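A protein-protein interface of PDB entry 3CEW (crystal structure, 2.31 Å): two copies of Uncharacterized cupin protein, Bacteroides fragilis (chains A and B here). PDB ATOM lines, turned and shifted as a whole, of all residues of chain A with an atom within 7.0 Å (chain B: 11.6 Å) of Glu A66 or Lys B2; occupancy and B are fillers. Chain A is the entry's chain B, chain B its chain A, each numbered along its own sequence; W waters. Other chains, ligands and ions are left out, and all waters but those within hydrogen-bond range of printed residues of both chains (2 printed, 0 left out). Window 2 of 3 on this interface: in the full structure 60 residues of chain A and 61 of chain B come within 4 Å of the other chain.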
ATOM      1  N   ILE A  61      21.458 -25.412  21.558  1.00  0.00           N
ATOM      2  CA  ILE A  61      20.455 -24.384  21.760  1.00  0.00           C
ATOM      3  C   ILE A  61      19.424 -24.602  20.660  1.00  0.00           C
ATOM      4  O   ILE A  61      19.767 -24.731  19.484  1.00  0.00           O
ATOM      5  CB  ILE A  61      21.031 -22.945  21.692  1.00  0.00           C
ATOM      6  CG1 ILE A  61      19.900 -21.945  21.939  1.00  0.00           C
ATOM      7  CG2 ILE A  61      21.700 -22.689  20.344  1.00  0.00           C
ATOM      8  CD1 ILE A  61      20.353 -20.487  22.009  1.00  0.00           C
ATOM      9  N   THR A  62      18.161 -24.691  21.048  1.00  0.00           N
ATOM     10  CA  THR A  62      17.107 -24.892  20.070  1.00  0.00           C
ATOM     11  C   THR A  62      16.446 -23.552  19.786  1.00  0.00           C
ATOM     12  O   THR A  62      15.939 -22.889  20.691  1.00  0.00           O
ATOM     13  CB  THR A  62      16.045 -25.895  20.571  1.00  0.00           C
ATOM     14  OG1 THR A  62      16.659 -27.166  20.797  1.00  0.00           O
ATOM     15  CG2 THR A  62      14.940 -26.071  19.539  1.00  0.00           C
ATOM     16  N   ILE A  63      16.477 -23.147  18.522  1.00  0.00           N
ATOM     17  CA  ILE A  63      15.878 -21.885  18.113  1.00  0.00           C
ATOM     18  C   ILE A  63      14.805 -22.165  17.067  1.00  0.00           C
ATOM     19  O   ILE A  63      15.098 -22.638  15.976  1.00  0.00           O
ATOM     20  CB  ILE A  63      16.950 -20.928  17.532  1.00  0.00           C
ATOM     21  CG1 ILE A  63      18.016 -20.640  18.595  1.00  0.00           C
ATOM     22  CG2 ILE A  63      16.303 -19.615  17.087  1.00  0.00           C
ATOM     23  CD1 ILE A  63      19.198 -19.833  18.074  1.00  0.00           C
ATOM     24  N   ASP A  64      13.558 -21.880  17.418  1.00  0.00           N
ATOM     25  CA  ASP A  64      12.429 -22.112  16.523  1.00  0.00           C
ATOM     26  C   ASP A  64      12.417 -23.544  15.955  1.00  0.00           C
ATOM     27  O   ASP A  64      12.336 -23.739  14.742  1.00  0.00           O
ATOM     28  CB  ASP A  64      12.445 -21.085  15.377  1.00  0.00           C
ATOM     29  CG  ASP A  64      12.250 -19.656  15.869  1.00  0.00           C
ATOM     30  OD1 ASP A  64      11.388 -19.440  16.747  1.00  0.00           O
ATOM     31  OD2 ASP A  64      12.946 -18.746  15.367  1.00  0.00           O
ATOM     32  N   GLY A  65      12.506 -24.537  16.839  1.00  0.00           N
ATOM     33  CA  GLY A  65      12.481 -25.931  16.416  1.00  0.00           C
ATOM     34  C   GLY A  65      13.793 -26.492  15.895  1.00  0.00           C
ATOM     35  O   GLY A  65      13.947 -27.707  15.750  1.00  0.00           O
ATOM     36  N   GLU A  66      14.750 -25.618  15.607  1.00  0.00           N
ATOM     37  CA  GLU A  66      16.040 -26.071  15.100  1.00  0.00           C
ATOM     38  C   GLU A  66      17.098 -26.068  16.198  1.00  0.00           C
ATOM     39  O   GLU A  66      17.348 -25.038  16.821  1.00  0.00           O
ATOM     40  CB  GLU A  66      16.496 -25.171  13.950  1.00  0.00           C
ATOM     41  CG  GLU A  66      17.802 -25.613  13.311  1.00  0.00           C
ATOM     42  CD  GLU A  66      18.334 -24.617  12.293  1.00  0.00           C
ATOM     43  OE1 GLU A  66      19.369 -24.915  11.663  1.00  0.00           O
ATOM     44  OE2 GLU A  66      17.723 -23.540  12.117  1.00  0.00           O
ATOM     45  N   LYS A  67      17.729 -27.212  16.439  1.00  0.00           N
ATOM     46  CA  LYS A  67      18.742 -27.249  17.480  1.00  0.00           C
ATOM     47  C   LYS A  67      20.138 -27.098  16.898  1.00  0.00           C
ATOM     48  O   LYS A  67      20.522 -27.799  15.956  1.00  0.00           O
ATOM     49  CB  LYS A  67      18.624 -28.525  18.323  1.00  0.00           C
ATOM     50  CG  LYS A  67      19.247 -29.763  17.737  1.00  0.00           C
ATOM     51  CD  LYS A  67      19.998 -30.532  18.823  1.00  0.00           C
ATOM     52  CE  LYS A  67      19.071 -30.989  19.948  1.00  0.00           C
ATOM     53  NZ  LYS A  67      19.794 -31.782  20.990  1.00  0.00           N
ATOM     54  N   ILE A  68      20.884 -26.155  17.462  1.00  0.00           N
ATOM     55  CA  ILE A  68      22.233 -25.857  17.009  1.00  0.00           C
ATOM     56  C   ILE A  68      23.255 -26.304  18.036  1.00  0.00           C
ATOM     57  O   ILE A  68      23.106 -26.041  19.230  1.00  0.00           O
ATOM     58  CB  ILE A  68      22.406 -24.347  16.802  1.00  0.00           C
ATOM     59  CG1 ILE A  68      21.226 -23.793  15.991  1.00  0.00           C
ATOM     60  CG2 ILE A  68      23.723 -24.067  16.117  1.00  0.00           C
ATOM     61  CD1 ILE A  68      21.013 -24.498  14.678  1.00  0.00           C
ATOM     62  N   ARG A  77      23.498 -14.306  17.683  1.00  0.00           N
ATOM     63  CA  ARG A  77      22.597 -13.182  17.803  1.00  0.00           C
ATOM     64  C   ARG A  77      21.239 -13.838  17.649  1.00  0.00           C
ATOM     65  O   ARG A  77      21.067 -14.714  16.803  1.00  0.00           O
ATOM     66  CB  ARG A  77      22.777 -12.174  16.668  1.00  0.00           C
ATOM     67  CG  ARG A  77      21.671 -11.111  16.633  1.00  0.00           C
ATOM     68  CD  ARG A  77      21.774 -10.211  15.399  1.00  0.00           C
ATOM     69  NE  ARG A  77      21.566 -10.968  14.166  1.00  0.00           N
ATOM     70  CZ  ARG A  77      20.376 -11.357  13.713  1.00  0.00           C
ATOM     71  NH1 ARG A  77      19.272 -11.050  14.381  1.00  0.00           N
ATOM     72  NH2 ARG A  77      20.292 -12.084  12.600  1.00  0.00           N
ATOM     73  N   ALA A  79      17.178 -12.816  17.226  1.00  0.00           N
ATOM     74  CA  ALA A  79      16.181 -11.764  17.088  1.00  0.00           C
ATOM     75  C   ALA A  79      15.089 -12.000  18.126  1.00  0.00           C
ATOM     76  O   ALA A  79      14.902 -13.123  18.597  1.00  0.00           O
ATOM     77  CB  ALA A  79      15.581 -11.777  15.669  1.00  0.00           C
ATOM     78  N   LYS A  83      12.329 -18.217  19.257  1.00  0.00           N
ATOM     79  CA  LYS A  83      11.964 -19.007  20.435  1.00  0.00           C
ATOM     80  C   LYS A  83      13.205 -19.833  20.747  1.00  0.00           C
ATOM     81  O   LYS A  83      13.603 -20.690  19.956  1.00  0.00           O
ATOM     82  CB  LYS A  83      10.780 -19.924  20.122  1.00  0.00           C
ATOM     83  CG  LYS A  83       9.488 -19.176  19.845  1.00  0.00           C
ATOM     84  CD  LYS A  83       8.346 -20.137  19.549  1.00  0.00           C
ATOM     85  CE  LYS A  83       7.062 -19.382  19.229  1.00  0.00           C
ATOM     86  NZ  LYS A  83       7.218 -18.487  18.042  1.00  0.00           N
ATOM     87  N   MET B   1      14.149 -14.891   6.582  1.00  0.00           N
ATOM     88  CA  MET B   1      15.317 -15.706   7.026  1.00  0.00           C
ATOM     89  C   MET B   1      15.257 -16.078   8.504  1.00  0.00           C
ATOM     90  O   MET B   1      14.313 -15.720   9.204  1.00  0.00           O
ATOM     91  CB  MET B   1      16.630 -14.974   6.705  1.00  0.00           C
ATOM     92  CG  MET B   1      16.512 -13.468   6.512  1.00  0.00           C
ATOM     93  SD  MET B   1      16.746 -12.414   8.120  1.00  0.00           S
ATOM     94  CE  MET B   1      18.593 -11.891   7.913  1.00  0.00           C
ATOM     95  N   LYS B   2      16.264 -16.811   8.965  1.00  0.00           N
ATOM     96  CA  LYS B   2      16.335 -17.267  10.354  1.00  0.00           C
ATOM     97  C   LYS B   2      16.362 -16.161  11.402  1.00  0.00           C
ATOM     98  O   LYS B   2      16.871 -15.069  11.156  1.00  0.00           O
ATOM     99  CB  LYS B   2      17.562 -18.160  10.538  1.00  0.00           C
ATOM    100  CG  LYS B   2      17.252 -19.640  10.630  1.00  0.00           C
ATOM    101  CD  LYS B   2      16.452 -20.147   9.445  1.00  0.00           C
ATOM    102  CE  LYS B   2      16.229 -21.645   9.573  1.00  0.00           C
ATOM    103  NZ  LYS B   2      15.386 -22.201   8.481  1.00  0.00           N
ATOM    104  N   ASN B   3      15.820 -16.465  12.580  1.00  0.00           N
ATOM    105  CA  ASN B   3      15.770 -15.513  13.683  1.00  0.00           C
ATOM    106  C   ASN B   3      17.078 -15.490  14.462  1.00  0.00           C
ATOM    107  O   ASN B   3      17.124 -15.016  15.598  1.00  0.00           O
ATOM    108  CB  ASN B   3      14.628 -15.860  14.636  1.00  0.00           C
ATOM    109  CG  ASN B   3      13.283 -15.355  14.152  1.00  0.00           C
ATOM    110  OD1 ASN B   3      12.271 -16.024  14.333  1.00  0.00           O
ATOM    111  ND2 ASN B   3      13.264 -14.166  13.551  1.00  0.00           N
ATOM    112  N   TYR B   4      18.144 -16.001  13.857  1.00  0.00           N
ATOM    113  CA  TYR B   4      19.441 -16.021  14.521  1.00  0.00           C
ATOM    114  C   TYR B   4      20.590 -16.131  13.524  1.00  0.00           C
ATOM    115  O   TYR B   4      20.390 -16.479  12.366  1.00  0.00           O
ATOM    116  CB  TYR B   4      19.533 -17.211  15.487  1.00  0.00           C
ATOM    117  CG  TYR B   4      19.823 -18.520  14.780  1.00  0.00           C
ATOM    118  CD1 TYR B   4      18.832 -19.180  14.055  1.00  0.00           C
ATOM    119  CD2 TYR B   4      21.116 -19.048  14.756  1.00  0.00           C
ATOM    120  CE1 TYR B   4      19.117 -20.325  13.321  1.00  0.00           C
ATOM    121  CE2 TYR B   4      21.417 -20.194  14.015  1.00  0.00           C
ATOM    122  CZ  TYR B   4      20.410 -20.825  13.300  1.00  0.00           C
ATOM    123  OH  TYR B   4      20.697 -21.941  12.546  1.00  0.00           O
ATOM    124  N   GLN B   5      21.790 -15.831  14.008  1.00  0.00           N
ATOM    125  CA  GLN B   5      23.028 -15.928  13.241  1.00  0.00           C
ATOM    126  C   GLN B   5      24.073 -16.458  14.212  1.00  0.00           C
ATOM    127  O   GLN B   5      24.063 -16.106  15.396  1.00  0.00           O
ATOM    128  CB  GLN B   5      23.473 -14.567  12.705  1.00  0.00           C
ATOM    129  CG  GLN B   5      22.737 -14.123  11.461  1.00  0.00           C
ATOM    130  CD  GLN B   5      23.273 -12.821  10.899  1.00  0.00           C
ATOM    131  OE1 GLN B   5      24.450 -12.720  10.553  1.00  0.00           O
ATOM    132  NE2 GLN B   5      22.408 -11.816  10.807  1.00  0.00           N
ATOM    133  N   LYS B   6      24.968 -17.302  13.710  1.00  0.00           N
ATOM    134  CA  LYS B   6      26.000 -17.902  14.542  1.00  0.00           C
ATOM    135  C   LYS B   6      27.368 -17.862  13.879  1.00  0.00           C
ATOM    136  O   LYS B   6      27.478 -17.808  12.659  1.00  0.00           O
ATOM    137  CB  LYS B   6      25.633 -19.358  14.845  1.00  0.00           C
ATOM    138  CG  LYS B   6      26.615 -20.089  15.754  1.00  0.00           C
ATOM    139  CD  LYS B   6      26.088 -21.471  16.135  1.00  0.00           C
ATOM    140  CE  LYS B   6      26.692 -22.573  15.277  1.00  0.00           C
ATOM    141  NZ  LYS B   6      28.047 -22.969  15.750  1.00  0.00           N
ATOM    142  N   SER B  20      29.585  -9.079  11.497  1.00  0.00           N
ATOM    143  CA  SER B  20      29.535 -10.521  11.254  1.00  0.00           C
ATOM    144  C   SER B  20      28.244 -11.184  11.732  1.00  0.00           C
ATOM    145  O   SER B  20      27.803 -12.178  11.154  1.00  0.00           O
ATOM    146  CB  SER B  20      30.730 -11.214  11.912  1.00  0.00           C
ATOM    147  OG  SER B  20      31.951 -10.780  11.338  1.00  0.00           O
ATOM    148  N   LEU B  21      27.648 -10.651  12.795  1.00  0.00           N
ATOM    149  CA  LEU B  21      26.403 -11.210  13.313  1.00  0.00           C
ATOM    150  C   LEU B  21      25.217 -10.300  13.038  1.00  0.00           C
ATOM    151  O   LEU B  21      24.093 -10.625  13.395  1.00  0.00           O
ATOM    152  CB  LEU B  21      26.507 -11.456  14.819  1.00  0.00           C
ATOM    153  CG  LEU B  21      27.427 -12.590  15.268  1.00  0.00           C
ATOM    154  CD1 LEU B  21      27.435 -12.665  16.787  1.00  0.00           C
ATOM    155  CD2 LEU B  21      26.939 -13.915  14.679  1.00  0.00           C
ATOM    156  N   ALA B  22      25.480  -9.161  12.401  1.00  0.00           N
ATOM    157  CA  ALA B  22      24.439  -8.184  12.077  1.00  0.00           C
ATOM    158  C   ALA B  22      23.712  -7.735  13.349  1.00  0.00           C
ATOM    159  O   ALA B  22      22.480  -7.730  13.407  1.00  0.00           O
ATOM    160  CB  ALA B  22      23.434  -8.779  11.070  1.00  0.00           C
ATOM    161  N   LEU B  23      24.476  -7.351  14.368  1.00  0.00           N
ATOM    162  CA  LEU B  23      23.884  -6.897  15.617  1.00  0.00           C
ATOM    163  C   LEU B  23      23.203  -5.551  15.381  1.00  0.00           C
ATOM    164  O   LEU B  23      23.611  -4.785  14.505  1.00  0.00           O
ATOM    165  CB  LEU B  23      24.964  -6.756  16.691  1.00  0.00           C
ATOM    166  CG  LEU B  23      25.771  -8.012  17.030  1.00  0.00           C
ATOM    167  CD1 LEU B  23      26.821  -7.683  18.100  1.00  0.00           C
ATOM    168  CD2 LEU B  23      24.828  -9.098  17.515  1.00  0.00           C
ATOM    169  N   THR B  24      22.155  -5.268  16.147  1.00  0.00           N
ATOM    170  CA  THR B  24      21.440  -4.005  15.999  1.00  0.00           C
ATOM    171  C   THR B  24      21.339  -3.287  17.337  1.00  0.00           C
ATOM    172  O   THR B  24      20.939  -2.131  17.396  1.00  0.00           O
ATOM    173  CB  THR B  24      20.000  -4.213  15.452  1.00  0.00           C
ATOM    174  OG1 THR B  24      19.216  -4.920  16.422  1.00  0.00           O
ATOM    175  CG2 THR B  24      20.024  -4.995  14.145  1.00  0.00           C
HETATM  176  O   HOH W   1      14.431 -19.113  13.452  1.00  0.00           O
HETATM  177  O   HOH W   2      17.446 -12.410  12.388  1.00  0.00           O
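Tyr B4 touches Ile A63. Glu A66 touches Lys B2. Ile A68 touches Tyr B4 (CD1 to OH, 3.3 Å). Ile A68 touches Lys B6. Tyr B4 touches Arg A77 (CA to O, 3.1 Å). Arg A77 touches Leu B23.
Glu A66 touches just these residues of chain B: Lys B2 and Tyr B4. Lys B2 touches just one residue of chain A: Glu A66. No residue of chain B comes within 4 Å of Thr A62. Printed residues of chain B within 4 Å of Ile A63: Tyr B4. Printed residues of chain B within 4 Å of Asp A64: Asn B3. No residue of chain B comes within 4 Å of Gly A65. Ile A68 touches just these residues of chain B: Tyr B4 and Lys B6. Of the printed residues of chain A, Gln B5 touches Arg A77 (2.8 Å). Printed residues of chain A within 4 Å of Leu B21: Arg A77 (2.7 Å). Of the printed residues of chain A, Ala B22 touches Arg A77 (3.3 Å). Of the printed residues of chain A, Asn B3 touches Asp A64 and Ala A79. Of the printed residues of chain A, Leu B23 touches Arg A77. Lys A83 touches none of the printed residues of chain B. Lys A67 touches none of the printed residues of chain B. The nearest residue of chain B that does not touch Glu A66 is Asn B3 (7.3 Å). The nearest residue of chain A that does not touch Lys B2 is Arg A77 (4.8 Å).
The side-chain amide oxygen (OD1) of Asn B3 sits close to the side-chain carboxylate (OD2) of Asp A64, 3.0 Å away. O of Asn B3 lies within hydrogen-bond range of N of Ala A79. OH of Tyr B4 sits at hydrogen-bond distance from OE1 of Glu A66, at 3.4 Å. The side-chain amide nitrogen (NE2) of Gln B5 lies close to the guanidinium group (NH2) of Arg A77 (2.8 Å). The backbone carbonyl oxygen (O) of Leu B21 lies within hydrogen-bond range of the guanidinium group (NE) of Arg A77, 2.7 Å away. O of Ala B22 sits close to NE of Arg A77, at 3.4 Å.
The side-chain amide oxygen (OE1) of Gln B5 sits close to the backbone carbonyl oxygen (O) of Ser B20. The side-chain amide nitrogen (NE2) of Gln B5 is in hydrogen-bond range of the backbone carbonyl oxygen (O) of Leu B21. O of Ile A61 sits at hydrogen-bond distance from N of Ile A68, 2.7 Å away. The backbone NH (N) of Asp A64 lies within hydrogen-bond range of the backbone carbonyl oxygen (O) of Lys A83 (2.8 Å).
Water W1 lies within hydrogen-bond range of the side-chain carboxylate (OD2) of Asp A64 (2.5 Å) and the backbone NH (N) of Asn B3 (3.1 Å). Water W2 lies within hydrogen-bond range of the guanidinium group of Arg A77 and the backbone carbonyl oxygen of Lys B2.
Of the 11 printed residues of chain A, 6 touch a printed residue of chain B. Hydrophobic or aromatic side chains of chain A within 4 Å of the printed part of chain B: Ile A63, Ile A68 and Ala A79. Printed residues of chain B that touch a printed residue of chain A: Lys B2, Asn B3, Tyr B4, Gln B5, Lys B6, Leu B21, Ala B22 and Leu B23. Along chain B the printed residues that touch a printed residue of chain A span positions 2 to 23. Among the printed residues, 12 pairs touch across the chains. Among the printed residues, no Asp or Glu carboxylate lies within 4 Å of a Lys or Arg side-chain nitrogen of the other chain.
No position is printed for both chains.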
